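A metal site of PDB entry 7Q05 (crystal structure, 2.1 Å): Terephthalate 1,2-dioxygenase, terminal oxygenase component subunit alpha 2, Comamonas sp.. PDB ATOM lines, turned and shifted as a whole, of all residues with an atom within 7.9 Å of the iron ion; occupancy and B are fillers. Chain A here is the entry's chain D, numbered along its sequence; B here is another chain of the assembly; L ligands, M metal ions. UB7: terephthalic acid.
OD1 of Asp 358 sits close to ND2 of Asn 206. The backbone carbonyl oxygen of Ile 354 sits close to a ring nitrogen (ND1) of His 217, at 2.8 Å. OE2 of Glu 357 is in hydrogen-bond range of ND1 of His 217 (2.6 Å). NE2 of His 212 sits close to OD1 of Asn 206, 3.4 Å away. A ring nitrogen (ND1) of His 212 is in hydrogen-bond range of the backbone carbonyl oxygen (O) of Asp 209 (2.8 Å). The side-chain hydroxyl (OH) of Tyr 106 of chain B is in hydrogen-bond range of the side-chain amide oxygen (OD1) of Asn 206, at 2.9 Å.
The iron ion is bound by OD1 of Asp 358 (2.3 Å), NE2 of His 217 (2.4 Å) and NE2 of His 212 (2.5 Å).
Asn 206 touches the iron ion (ND2 to FE, 3.7 Å). Within 4 Å of the iron ion: Asn 206, His 212, His 217 and Asp 358. The nearest printed residue that does not touch the iron ion is Leu 216 (4.7 Å).
The guanidinium group (NH2) of Arg 311 is in salt-bridge range of an oxygen (O12) of the ligand, at 2.7 Å.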
ATOM      1  N   TYR A 203      30.222  19.519  37.231  1.00  0.00           N
ATOM      2  CA  TYR A 203      28.850  19.623  36.684  1.00  0.00           C
ATOM      3  C   TYR A 203      28.640  21.033  36.121  1.00  0.00           C
ATOM      4  O   TYR A 203      28.085  21.144  35.027  1.00  0.00           O
ATOM      5  CB  TYR A 203      27.740  19.245  37.666  1.00  0.00           C
ATOM      6  CG  TYR A 203      26.394  19.337  36.984  1.00  0.00           C
ATOM      7  CD1 TYR A 203      25.903  18.343  36.157  1.00  0.00           C
ATOM      8  CD2 TYR A 203      25.633  20.485  37.117  1.00  0.00           C
ATOM      9  CE1 TYR A 203      24.659  18.448  35.552  1.00  0.00           C
ATOM     10  CE2 TYR A 203      24.428  20.642  36.464  1.00  0.00           C
ATOM     11  CZ  TYR A 203      23.922  19.612  35.708  1.00  0.00           C
ATOM     12  OH  TYR A 203      22.717  19.783  35.094  1.00  0.00           O
ATOM     13  N   ASN A 206      30.208  21.273  32.930  1.00  0.00           N
ATOM     14  CA  ASN A 206      29.453  20.433  31.960  1.00  0.00           C
ATOM     15  C   ASN A 206      28.295  21.262  31.393  1.00  0.00           C
ATOM     16  O   ASN A 206      28.069  21.199  30.189  1.00  0.00           O
ATOM     17  CB  ASN A 206      28.929  19.139  32.574  1.00  0.00           C
ATOM     18  CG  ASN A 206      28.293  18.244  31.533  1.00  0.00           C
ATOM     19  OD1 ASN A 206      28.990  17.735  30.667  1.00  0.00           O
ATOM     20  ND2 ASN A 206      26.982  18.142  31.524  1.00  0.00           N
ATOM     21  N   VAL A 207      27.609  22.032  32.227  1.00  0.00           N
ATOM     22  CA  VAL A 207      26.432  22.836  31.784  1.00  0.00           C
ATOM     23  C   VAL A 207      26.913  23.843  30.726  1.00  0.00           C
ATOM     24  O   VAL A 207      26.151  24.160  29.805  1.00  0.00           O
ATOM     25  CB  VAL A 207      25.767  23.577  32.963  1.00  0.00           C
ATOM     26  CG1 VAL A 207      24.630  24.415  32.425  1.00  0.00           C
ATOM     27  CG2 VAL A 207      25.226  22.662  34.017  1.00  0.00           C
ATOM     28  N   LYS A 208      28.127  24.374  30.914  1.00  0.00           N
ATOM     29  CA  LYS A 208      28.730  25.446  30.065  1.00  0.00           C
ATOM     30  C   LYS A 208      29.445  24.823  28.867  1.00  0.00           C
ATOM     31  O   LYS A 208      30.015  25.600  28.038  1.00  0.00           O
ATOM     32  CB  LYS A 208      29.666  26.308  30.912  1.00  0.00           C
ATOM     33  CG  LYS A 208      29.022  27.039  32.072  1.00  0.00           C
ATOM     34  CD  LYS A 208      30.007  27.610  33.047  1.00  0.00           C
ATOM     35  CE  LYS A 208      29.352  28.469  34.118  1.00  0.00           C
ATOM     36  NZ  LYS A 208      28.767  29.685  33.508  1.00  0.00           N
ATOM     37  N   ASP A 209      29.419  23.499  28.735  1.00  0.00           N
ATOM     38  CA  ASP A 209      30.316  22.802  27.779  1.00  0.00           C
ATOM     39  C   ASP A 209      29.565  22.630  26.464  1.00  0.00           C
ATOM     40  O   ASP A 209      29.091  21.522  26.203  1.00  0.00           O
ATOM     41  CB  ASP A 209      30.917  21.558  28.417  1.00  0.00           C
ATOM     42  CG  ASP A 209      31.942  20.801  27.604  1.00  0.00           C
ATOM     43  OD1 ASP A 209      32.167  21.143  26.428  1.00  0.00           O
ATOM     44  OD2 ASP A 209      32.471  19.855  28.146  1.00  0.00           O
ATOM     45  N   HIS A 212      30.715  19.510  24.229  1.00  0.00           N
ATOM     46  CA  HIS A 212      30.194  18.160  24.547  1.00  0.00           C
ATOM     47  C   HIS A 212      28.768  17.956  24.044  1.00  0.00           C
ATOM     48  O   HIS A 212      28.459  16.780  23.668  1.00  0.00           O
ATOM     49  CB  HIS A 212      30.386  17.868  26.034  1.00  0.00           C
ATOM     50  CG  HIS A 212      29.126  17.843  26.786  1.00  0.00           C
ATOM     51  ND1 HIS A 212      28.582  18.997  27.345  1.00  0.00           N
ATOM     52  CD2 HIS A 212      28.307  16.815  27.049  1.00  0.00           C
ATOM     53  CE1 HIS A 212      27.455  18.671  27.942  1.00  0.00           C
ATOM     54  NE2 HIS A 212      27.278  17.309  27.777  1.00  0.00           N
ATOM     55  N   ALA A 213      27.874  18.962  24.040  1.00  0.00           N
ATOM     56  CA  ALA A 213      26.396  18.770  23.829  1.00  0.00           C
ATOM     57  C   ALA A 213      26.041  17.701  22.777  1.00  0.00           C
ATOM     58  O   ALA A 213      25.290  16.762  23.108  1.00  0.00           O
ATOM     59  CB  ALA A 213      25.732  20.055  23.479  1.00  0.00           C
ATOM     60  N   SER A 214      26.594  17.788  21.565  1.00  0.00           N
ATOM     61  CA  SER A 214      26.264  16.932  20.402  1.00  0.00           C
ATOM     62  C   SER A 214      27.030  15.606  20.415  1.00  0.00           C
ATOM     63  O   SER A 214      26.644  14.687  19.662  1.00  0.00           O
ATOM     64  CB  SER A 214      26.496  17.711  19.106  1.00  0.00           C
ATOM     65  OG  SER A 214      27.865  18.016  18.915  1.00  0.00           O
ATOM     66  N   LEU A 216      28.669  13.749  23.538  1.00  0.00           N
ATOM     67  CA  LEU A 216      28.165  12.927  24.660  1.00  0.00           C
ATOM     68  C   LEU A 216      26.738  12.420  24.368  1.00  0.00           C
ATOM     69  O   LEU A 216      26.464  11.225  24.616  1.00  0.00           O
ATOM     70  CB  LEU A 216      28.195  13.784  25.931  1.00  0.00           C
ATOM     71  CG  LEU A 216      27.679  13.064  27.180  1.00  0.00           C
ATOM     72  CD1 LEU A 216      28.479  11.795  27.461  1.00  0.00           C
ATOM     73  CD2 LEU A 216      27.675  14.019  28.357  1.00  0.00           C
ATOM     74  N   HIS A 217      25.851  13.299  23.865  1.00  0.00           N
ATOM     75  CA  HIS A 217      24.397  13.034  23.661  1.00  0.00           C
ATOM     76  C   HIS A 217      24.074  12.703  22.196  1.00  0.00           C
ATOM     77  O   HIS A 217      23.891  13.668  21.376  1.00  0.00           O
ATOM     78  CB  HIS A 217      23.565  14.221  24.131  1.00  0.00           C
ATOM     79  CG  HIS A 217      23.950  14.716  25.478  1.00  0.00           C
ATOM     80  ND1 HIS A 217      24.005  13.865  26.569  1.00  0.00           N
ATOM     81  CD2 HIS A 217      24.247  15.946  25.927  1.00  0.00           C
ATOM     82  CE1 HIS A 217      24.309  14.568  27.640  1.00  0.00           C
ATOM     83  NE2 HIS A 217      24.463  15.851  27.277  1.00  0.00           N
ATOM     84  N   PHE A 220      20.946  14.455  20.863  1.00  0.00           N
ATOM     85  CA  PHE A 220      21.184  15.848  20.378  1.00  0.00           C
ATOM     86  C   PHE A 220      21.649  15.881  18.900  1.00  0.00           C
ATOM     87  O   PHE A 220      21.298  16.857  18.205  1.00  0.00           O
ATOM     88  CB  PHE A 220      22.210  16.592  21.253  1.00  0.00           C
ATOM     89  CG  PHE A 220      21.680  17.522  22.328  1.00  0.00           C
ATOM     90  CD1 PHE A 220      20.422  18.099  22.245  1.00  0.00           C
ATOM     91  CD2 PHE A 220      22.474  17.846  23.414  1.00  0.00           C
ATOM     92  CE1 PHE A 220      19.967  18.943  23.248  1.00  0.00           C
ATOM     93  CE2 PHE A 220      22.027  18.706  24.407  1.00  0.00           C
ATOM     94  CZ  PHE A 220      20.765  19.251  24.333  1.00  0.00           C
ATOM     95  N   ILE A 292      20.177  27.056  27.066  1.00  0.00           N
ATOM     96  CA  ILE A 292      20.727  26.725  28.393  1.00  0.00           C
ATOM     97  C   ILE A 292      21.400  27.978  28.924  1.00  0.00           C
ATOM     98  O   ILE A 292      22.281  28.528  28.245  1.00  0.00           O
ATOM     99  CB  ILE A 292      21.723  25.558  28.310  1.00  0.00           C
ATOM    100  CG1 ILE A 292      21.152  24.400  27.509  1.00  0.00           C
ATOM    101  CG2 ILE A 292      22.064  25.092  29.727  1.00  0.00           C
ATOM    102  CD1 ILE A 292      19.973  23.736  28.203  1.00  0.00           C
ATOM    103  N   ARG A 311      17.545  24.374  37.501  1.00  0.00           N
ATOM    104  CA  ARG A 311      18.427  23.494  38.313  1.00  0.00           C
ATOM    105  C   ARG A 311      19.185  24.325  39.312  1.00  0.00           C
ATOM    106  O   ARG A 311      19.644  25.426  38.965  1.00  0.00           O
ATOM    107  CB  ARG A 311      19.416  22.715  37.458  1.00  0.00           C
ATOM    108  CG  ARG A 311      18.813  22.259  36.142  1.00  0.00           C
ATOM    109  CD  ARG A 311      19.833  21.578  35.283  1.00  0.00           C
ATOM    110  NE  ARG A 311      19.350  21.491  33.927  1.00  0.00           N
ATOM    111  CZ  ARG A 311      20.105  21.323  32.855  1.00  0.00           C
ATOM    112  NH1 ARG A 311      19.506  21.207  31.681  1.00  0.00           N
ATOM    113  NH2 ARG A 311      21.437  21.206  32.941  1.00  0.00           N
ATOM    114  N   ILE A 354      18.682  12.924  27.125  1.00  0.00           N
ATOM    115  CA  ILE A 354      19.839  13.858  27.034  1.00  0.00           C
ATOM    116  C   ILE A 354      20.612  13.807  28.343  1.00  0.00           C
ATOM    117  O   ILE A 354      21.833  13.533  28.324  1.00  0.00           O
ATOM    118  CB  ILE A 354      19.395  15.310  26.749  1.00  0.00           C
ATOM    119  CG1 ILE A 354      18.754  15.447  25.374  1.00  0.00           C
ATOM    120  CG2 ILE A 354      20.556  16.285  26.938  1.00  0.00           C
ATOM    121  CD1 ILE A 354      19.432  14.571  24.395  1.00  0.00           C
ATOM    122  N   SER A 355      19.984  14.121  29.455  1.00  0.00           N
ATOM    123  CA  SER A 355      20.763  14.557  30.639  1.00  0.00           C
ATOM    124  C   SER A 355      21.264  13.397  31.504  1.00  0.00           C
ATOM    125  O   SER A 355      22.003  13.676  32.482  1.00  0.00           O
ATOM    126  CB  SER A 355      19.983  15.564  31.427  1.00  0.00           C
ATOM    127  OG  SER A 355      18.705  15.089  31.646  1.00  0.00           O
ATOM    128  N   MET A 356      20.843  12.163  31.210  1.00  0.00           N
ATOM    129  CA  MET A 356      21.231  10.953  31.975  1.00  0.00           C
ATOM    130  C   MET A 356      22.760  10.936  32.028  1.00  0.00           C
ATOM    131  O   MET A 356      23.299  10.801  33.092  1.00  0.00           O
ATOM    132  CB  MET A 356      20.688   9.725  31.227  1.00  0.00           C
ATOM    133  CG  MET A 356      21.035   8.443  31.734  1.00  0.00           C
ATOM    134  SD  MET A 356      20.464   7.134  30.685  1.00  0.00           S
ATOM    135  CE  MET A 356      18.699   7.360  30.653  1.00  0.00           C
ATOM    136  N   GLU A 357      23.421  11.101  30.876  1.00  0.00           N
ATOM    137  CA  GLU A 357      24.881  11.116  30.691  1.00  0.00           C
ATOM    138  C   GLU A 357      25.515  12.227  31.527  1.00  0.00           C
ATOM    139  O   GLU A 357      26.564  11.995  32.086  1.00  0.00           O
ATOM    140  CB  GLU A 357      25.214  11.316  29.227  1.00  0.00           C
ATOM    141  CG  GLU A 357      24.850  10.102  28.419  1.00  0.00           C
ATOM    142  CD  GLU A 357      23.738  10.286  27.387  1.00  0.00           C
ATOM    143  OE1 GLU A 357      23.387   9.291  26.703  1.00  0.00           O
ATOM    144  OE2 GLU A 357      23.346  11.432  27.170  1.00  0.00           O
ATOM    145  N   ASP A 358      24.883  13.410  31.615  1.00  0.00           N
ATOM    146  CA  ASP A 358      25.424  14.557  32.377  1.00  0.00           C
ATOM    147  C   ASP A 358      25.564  14.126  33.849  1.00  0.00           C
ATOM    148  O   ASP A 358      26.449  14.601  34.527  1.00  0.00           O
ATOM    149  CB  ASP A 358      24.575  15.815  32.237  1.00  0.00           C
ATOM    150  CG  ASP A 358      24.364  16.304  30.818  1.00  0.00           C
ATOM    151  OD1 ASP A 358      25.379  16.242  30.023  1.00  0.00           O
ATOM    152  OD2 ASP A 358      23.185  16.777  30.521  1.00  0.00           O
ATOM    153  N   GLY A 359      24.703  13.257  34.359  1.00  0.00           N
ATOM    154  CA  GLY A 359      24.843  12.793  35.744  1.00  0.00           C
ATOM    155  C   GLY A 359      26.089  11.908  35.960  1.00  0.00           C
ATOM    156  O   GLY A 359      26.579  11.871  37.097  1.00  0.00           O
ATOM    157  N   VAL A 361      29.121  11.860  33.657  1.00  0.00           N
ATOM    158  CA  VAL A 361      30.407  12.266  33.008  1.00  0.00           C
ATOM    159  C   VAL A 361      31.291  12.915  34.062  1.00  0.00           C
ATOM    160  O   VAL A 361      32.476  12.682  33.961  1.00  0.00           O
ATOM    161  CB  VAL A 361      30.337  13.189  31.780  1.00  0.00           C
ATOM    162  CG1 VAL A 361      29.895  12.444  30.581  1.00  0.00           C
ATOM    163  CG2 VAL A 361      29.516  14.442  32.006  1.00  0.00           C
ATOM    164  N   TYR B 106      32.957  11.707  26.366  1.00  0.00           N
ATOM    165  CA  TYR B 106      32.642  13.120  26.744  1.00  0.00           C
ATOM    166  C   TYR B 106      32.711  14.004  25.503  1.00  0.00           C
ATOM    167  O   TYR B 106      31.711  14.649  25.190  1.00  0.00           O
ATOM    168  CB  TYR B 106      33.584  13.584  27.860  1.00  0.00           C
ATOM    169  CG  TYR B 106      33.058  14.689  28.731  1.00  0.00           C
ATOM    170  CD1 TYR B 106      31.944  15.424  28.408  1.00  0.00           C
ATOM    171  CD2 TYR B 106      33.733  15.015  29.886  1.00  0.00           C
ATOM    172  CE1 TYR B 106      31.542  16.486  29.211  1.00  0.00           C
ATOM    173  CE2 TYR B 106      33.304  16.023  30.725  1.00  0.00           C
ATOM    174  CZ  TYR B 106      32.201  16.782  30.387  1.00  0.00           C
ATOM    175  OH  TYR B 106      31.785  17.754  31.259  1.00  0.00           O
HETATM  176  C01 UB7 L   1      24.779  22.522  27.366  1.00  0.00           C
HETATM  177  C02 UB7 L   1      24.178  21.906  28.451  1.00  0.00           C
HETATM  178  C03 UB7 L   1      22.944  21.236  28.314  1.00  0.00           C
HETATM  179  C04 UB7 L   1      22.357  21.171  27.049  1.00  0.00           C
HETATM  180  C05 UB7 L   1      22.944  21.802  25.956  1.00  0.00           C
HETATM  181  C06 UB7 L   1      24.165  22.497  26.102  1.00  0.00           C
HETATM  182  C07 UB7 L   1      24.772  23.276  24.973  1.00  0.00           C
HETATM  183  C10 UB7 L   1      22.246  20.705  29.533  1.00  0.00           C
HETATM  184  O08 UB7 L   1      25.612  24.169  25.207  1.00  0.00           O
HETATM  185  O09 UB7 L   1      24.363  22.969  23.772  1.00  0.00           O
HETATM  186  O11 UB7 L   1      21.016  20.202  29.316  1.00  0.00           O
HETATM  187  O12 UB7 L   1      22.787  20.747  30.687  1.00  0.00           O
HETATM  188 FE    FE M   1      24.942  17.836  28.469  1.00  0.00          FE
